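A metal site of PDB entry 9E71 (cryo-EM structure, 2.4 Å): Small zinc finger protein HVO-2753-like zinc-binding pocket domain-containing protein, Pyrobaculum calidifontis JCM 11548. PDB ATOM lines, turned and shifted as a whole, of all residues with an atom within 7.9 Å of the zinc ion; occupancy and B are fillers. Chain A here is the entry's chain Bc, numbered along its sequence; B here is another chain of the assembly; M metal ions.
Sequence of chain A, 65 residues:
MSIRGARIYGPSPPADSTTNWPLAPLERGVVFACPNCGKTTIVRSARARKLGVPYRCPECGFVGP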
ATOM      1  N   ALA A  33     -12.038  -5.444 -14.232  1.00  0.00           N
ATOM      2  CA  ALA A  33     -12.462  -4.104 -14.618  1.00  0.00           C
ATOM      3  C   ALA A  33     -11.239  -3.265 -14.945  1.00  0.00           C
ATOM      4  O   ALA A  33     -10.122  -3.603 -14.543  1.00  0.00           O
ATOM      5  CB  ALA A  33     -13.278  -3.445 -13.512  1.00  0.00           C
ATOM      6  N   CYS A  34     -11.458  -2.171 -15.668  1.00  0.00           N
ATOM      7  CA  CYS A  34     -10.366  -1.311 -16.108  1.00  0.00           C
ATOM      8  C   CYS A  34      -9.616  -0.719 -14.924  1.00  0.00           C
ATOM      9  O   CYS A  34     -10.221  -0.083 -14.056  1.00  0.00           O
ATOM     10  CB  CYS A  34     -10.870  -0.179 -17.001  1.00  0.00           C
ATOM     11  SG  CYS A  34      -9.599   1.045 -17.383  1.00  0.00           S
ATOM     12  N   PRO A  35      -8.300  -0.953 -14.837  1.00  0.00           N
ATOM     13  CA  PRO A  35      -7.534  -0.424 -13.692  1.00  0.00           C
ATOM     14  C   PRO A  35      -7.537   1.088 -13.593  1.00  0.00           C
ATOM     15  O   PRO A  35      -7.468   1.620 -12.481  1.00  0.00           O
ATOM     16  CB  PRO A  35      -6.125  -0.976 -13.946  1.00  0.00           C
ATOM     17  CG  PRO A  35      -6.359  -2.208 -14.752  1.00  0.00           C
ATOM     18  CD  PRO A  35      -7.498  -1.862 -15.662  1.00  0.00           C
ATOM     19  N   ASN A  36      -7.633   1.801 -14.712  1.00  0.00           N
ATOM     20  CA  ASN A  36      -7.634   3.254 -14.653  1.00  0.00           C
ATOM     21  C   ASN A  36      -9.012   3.798 -14.284  1.00  0.00           C
ATOM     22  O   ASN A  36      -9.136   4.627 -13.382  1.00  0.00           O
ATOM     23  CB  ASN A  36      -7.174   3.837 -15.985  1.00  0.00           C
ATOM     24  CG  ASN A  36      -7.197   5.344 -15.997  1.00  0.00           C
ATOM     25  OD1 ASN A  36      -6.770   5.990 -15.047  1.00  0.00           O
ATOM     26  ND2 ASN A  36      -7.704   5.918 -17.084  1.00  0.00           N
ATOM     27  N   CYS A  37     -10.064   3.331 -14.967  1.00  0.00           N
ATOM     28  CA  CYS A  37     -11.436   3.740 -14.662  1.00  0.00           C
ATOM     29  C   CYS A  37     -12.171   2.744 -13.778  1.00  0.00           C
ATOM     30  O   CYS A  37     -12.656   3.108 -12.712  1.00  0.00           O
ATOM     31  CB  CYS A  37     -12.252   3.940 -15.945  1.00  0.00           C
ATOM     32  SG  CYS A  37     -11.343   4.503 -17.389  1.00  0.00           S
ATOM     33  N   GLY A  38     -12.245   1.491 -14.194  1.00  0.00           N
ATOM     34  CA  GLY A  38     -13.112   0.526 -13.571  1.00  0.00           C
ATOM     35  C   GLY A  38     -14.487   0.426 -14.188  1.00  0.00           C
ATOM     36  O   GLY A  38     -15.334  -0.311 -13.673  1.00  0.00           O
ATOM     37  N   LYS A  39     -14.736   1.140 -15.289  1.00  0.00           N
ATOM     38  CA  LYS A  39     -16.047   1.123 -15.910  1.00  0.00           C
ATOM     39  C   LYS A  39     -16.192  -0.025 -16.897  1.00  0.00           C
ATOM     40  O   LYS A  39     -17.072  -0.877 -16.730  1.00  0.00           O
ATOM     41  CB  LYS A  39     -16.319   2.460 -16.607  1.00  0.00           C
ATOM     42  CG  LYS A  39     -15.963   3.659 -15.751  1.00  0.00           C
ATOM     43  CD  LYS A  39     -17.136   4.046 -14.861  1.00  0.00           C
ATOM     44  CE  LYS A  39     -16.885   5.367 -14.157  1.00  0.00           C
ATOM     45  NZ  LYS A  39     -16.717   6.476 -15.137  1.00  0.00           N
ATOM     46  N   THR A  40     -15.348  -0.063 -17.917  1.00  0.00           N
ATOM     47  CA  THR A  40     -15.394  -1.134 -18.900  1.00  0.00           C
ATOM     48  C   THR A  40     -14.752  -2.392 -18.332  1.00  0.00           C
ATOM     49  O   THR A  40     -13.970  -2.338 -17.382  1.00  0.00           O
ATOM     50  CB  THR A  40     -14.663  -0.718 -20.180  1.00  0.00           C
ATOM     51  OG1 THR A  40     -14.843   0.684 -20.393  1.00  0.00           O
ATOM     52  CG2 THR A  40     -15.219  -1.476 -21.360  1.00  0.00           C
ATOM     53  N   ILE A  42     -12.329  -5.771 -18.919  1.00  0.00           N
ATOM     54  CA  ILE A  42     -11.168  -6.224 -19.671  1.00  0.00           C
ATOM     55  C   ILE A  42     -11.136  -7.751 -19.591  1.00  0.00           C
ATOM     56  O   ILE A  42     -11.122  -8.320 -18.490  1.00  0.00           O
ATOM     57  CB  ILE A  42      -9.867  -5.613 -19.140  1.00  0.00           C
ATOM     58  CG1 ILE A  42      -9.928  -4.094 -19.260  1.00  0.00           C
ATOM     59  CG2 ILE A  42      -8.679  -6.171 -19.892  1.00  0.00           C
ATOM     60  CD1 ILE A  42     -10.122  -3.612 -20.672  1.00  0.00           C
ATOM     61  N   ARG A  56      -6.520  -2.091 -24.422  1.00  0.00           N
ATOM     62  CA  ARG A  56      -6.836  -0.681 -24.387  1.00  0.00           C
ATOM     63  C   ARG A  56      -8.240  -0.480 -23.845  1.00  0.00           C
ATOM     64  O   ARG A  56      -9.150  -1.262 -24.170  1.00  0.00           O
ATOM     65  CB  ARG A  56      -6.715  -0.063 -25.787  1.00  0.00           C
ATOM     66  CG  ARG A  56      -5.787   1.125 -25.854  1.00  0.00           C
ATOM     67  CD  ARG A  56      -5.942   1.877 -27.165  1.00  0.00           C
ATOM     68  NE  ARG A  56      -7.048   2.824 -27.181  1.00  0.00           N
ATOM     69  CZ  ARG A  56      -7.170   3.870 -26.367  1.00  0.00           C
ATOM     70  NH1 ARG A  56      -6.237   4.188 -25.493  1.00  0.00           N
ATOM     71  NH2 ARG A  56      -8.261   4.632 -26.452  1.00  0.00           N
ATOM     72  N   CYS A  57      -8.420   0.539 -23.025  1.00  0.00           N
ATOM     73  CA  CYS A  57      -9.752   0.858 -22.530  1.00  0.00           C
ATOM     74  C   CYS A  57     -10.550   1.553 -23.628  1.00  0.00           C
ATOM     75  O   CYS A  57     -10.047   2.486 -24.254  1.00  0.00           O
ATOM     76  CB  CYS A  57      -9.698   1.738 -21.296  1.00  0.00           C
ATOM     77  SG  CYS A  57     -11.327   2.085 -20.574  1.00  0.00           S
ATOM     78  N   PRO A  58     -11.787   1.116 -23.895  1.00  0.00           N
ATOM     79  CA  PRO A  58     -12.630   1.883 -24.835  1.00  0.00           C
ATOM     80  C   PRO A  58     -12.979   3.266 -24.320  1.00  0.00           C
ATOM     81  O   PRO A  58     -13.247   4.174 -25.130  1.00  0.00           O
ATOM     82  CB  PRO A  58     -13.875   0.994 -24.994  1.00  0.00           C
ATOM     83  CG  PRO A  58     -13.664  -0.215 -24.145  1.00  0.00           C
ATOM     84  CD  PRO A  58     -12.506   0.011 -23.252  1.00  0.00           C
ATOM     85  N   GLU A  59     -12.992   3.468 -23.005  1.00  0.00           N
ATOM     86  CA  GLU A  59     -13.340   4.762 -22.434  1.00  0.00           C
ATOM     87  C   GLU A  59     -12.112   5.625 -22.181  1.00  0.00           C
ATOM     88  O   GLU A  59     -12.051   6.760 -22.650  1.00  0.00           O
ATOM     89  CB  GLU A  59     -14.131   4.561 -21.147  1.00  0.00           C
ATOM     90  CG  GLU A  59     -15.303   3.612 -21.273  1.00  0.00           C
ATOM     91  CD  GLU A  59     -16.212   3.641 -20.064  1.00  0.00           C
ATOM     92  OE1 GLU A  59     -15.823   4.254 -19.054  1.00  0.00           O
ATOM     93  OE2 GLU A  59     -17.304   3.037 -20.127  1.00  0.00           O
ATOM     94  N   CYS A  60     -11.145   5.116 -21.434  1.00  0.00           N
ATOM     95  CA  CYS A  60      -9.931   5.863 -21.122  1.00  0.00           C
ATOM     96  C   CYS A  60      -8.795   5.408 -22.038  1.00  0.00           C
ATOM     97  O   CYS A  60      -8.903   4.384 -22.710  1.00  0.00           O
ATOM     98  CB  CYS A  60      -9.523   5.675 -19.666  1.00  0.00           C
ATOM     99  SG  CYS A  60      -8.556   4.194 -19.361  1.00  0.00           S
ATOM    100  N   GLY A  61      -7.714   6.170 -22.055  1.00  0.00           N
ATOM    101  CA  GLY A  61      -6.566   5.840 -22.867  1.00  0.00           C
ATOM    102  C   GLY A  61      -5.480   5.063 -22.141  1.00  0.00           C
ATOM    103  O   GLY A  61      -4.303   5.423 -22.228  1.00  0.00           O
ATOM    104  N   PHE A  62      -5.850   3.996 -21.436  1.00  0.00           N
ATOM    105  CA  PHE A  62      -4.897   3.217 -20.657  1.00  0.00           C
ATOM    106  C   PHE A  62      -4.616   1.900 -21.358  1.00  0.00           C
ATOM    107  O   PHE A  62      -5.534   1.170 -21.725  1.00  0.00           O
ATOM    108  CB  PHE A  62      -5.437   2.947 -19.247  1.00  0.00           C
ATOM    109  CG  PHE A  62      -4.671   1.899 -18.484  1.00  0.00           C
ATOM    110  CD1 PHE A  62      -3.451   2.199 -17.902  1.00  0.00           C
ATOM    111  CD2 PHE A  62      -5.185   0.626 -18.321  1.00  0.00           C
ATOM    112  CE1 PHE A  62      -2.756   1.242 -17.206  1.00  0.00           C
ATOM    113  CE2 PHE A  62      -4.496  -0.328 -17.619  1.00  0.00           C
ATOM    114  CZ  PHE A  62      -3.273  -0.014 -17.057  1.00  0.00           C
ATOM    115  N   VAL A  63      -3.331   1.598 -21.524  1.00  0.00           N
ATOM    116  CA  VAL A  63      -2.863   0.346 -22.110  1.00  0.00           C
ATOM    117  C   VAL A  63      -2.127  -0.427 -21.024  1.00  0.00           C
ATOM    118  O   VAL A  63      -1.132   0.058 -20.473  1.00  0.00           O
ATOM    119  CB  VAL A  63      -1.958   0.582 -23.319  1.00  0.00           C
ATOM    120  CG1 VAL A  63      -2.771   0.891 -24.545  1.00  0.00           C
ATOM    121  CG2 VAL A  63      -0.967   1.703 -23.033  1.00  0.00           C
ATOM    122  N   ARG B  67     -10.616  -1.651  -5.424  1.00  0.00           N
ATOM    123  CA  ARG B  67     -11.909  -2.156  -5.873  1.00  0.00           C
ATOM    124  C   ARG B  67     -12.183  -3.590  -5.461  1.00  0.00           C
ATOM    125  O   ARG B  67     -13.295  -4.073  -5.681  1.00  0.00           O
ATOM    126  CB  ARG B  67     -12.020  -2.011  -7.392  1.00  0.00           C
ATOM    127  CG  ARG B  67     -12.366  -0.593  -7.812  1.00  0.00           C
ATOM    128  CD  ARG B  67     -12.398  -0.449  -9.313  1.00  0.00           C
ATOM    129  NE  ARG B  67     -11.061  -0.630  -9.874  1.00  0.00           N
ATOM    130  CZ  ARG B  67     -10.460   0.236 -10.670  1.00  0.00           C
ATOM    131  NH1 ARG B  67     -11.060   1.353 -11.061  1.00  0.00           N
ATOM    132  NH2 ARG B  67      -9.224  -0.017 -11.085  1.00  0.00           N
HETATM  133 ZN    ZN M   1     -10.304   2.863 -18.645  1.00  0.00          ZN
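The zinc ion is bound by the side-chain sulfur of Cys 60 (2.3 Å), the side-chain sulfur of Cys 37 (2.3 Å), the side-chain sulfur of Cys 57 (2.3 Å) and the side-chain sulfur of Cys 34 (2.3 Å).
Within 4 Å of the zinc ion: Cys 34, Cys 37, Cys 57 and Cys 60.
The nearest printed residue that does not touch the zinc ion is Asn 36 (4.2 Å).
The backbone carbonyl oxygen (O) of Thr 40 sits at hydrogen-bond distance from the backbone NH (N) of Cys 34, at 3.0 Å.
N of Phe 62 lies close to SG of Cys 60 (3.4 Å).
O of Cys 34 is in hydrogen-bond range of NH2 of Arg 67 of chain B, 3.1 Å away.
The side-chain sulfur (SG) of Cys 57 lies close to the side-chain hydroxyl (OG1) of Thr 40, at 3.8 Å.
The backbone carbonyl oxygen of Phe 62 sits at hydrogen-bond distance from the backbone NH of Cys 57, 3.2 Å away.
SG of Cys 34 sits close to N of Asn 36, at 3.4 Å.
O of Cys 37 is in hydrogen-bond range of NH1 of Arg 67 of chain B (2.9 Å).
SG of Cys 57 sits close to N of Glu 59 (3.3 Å).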
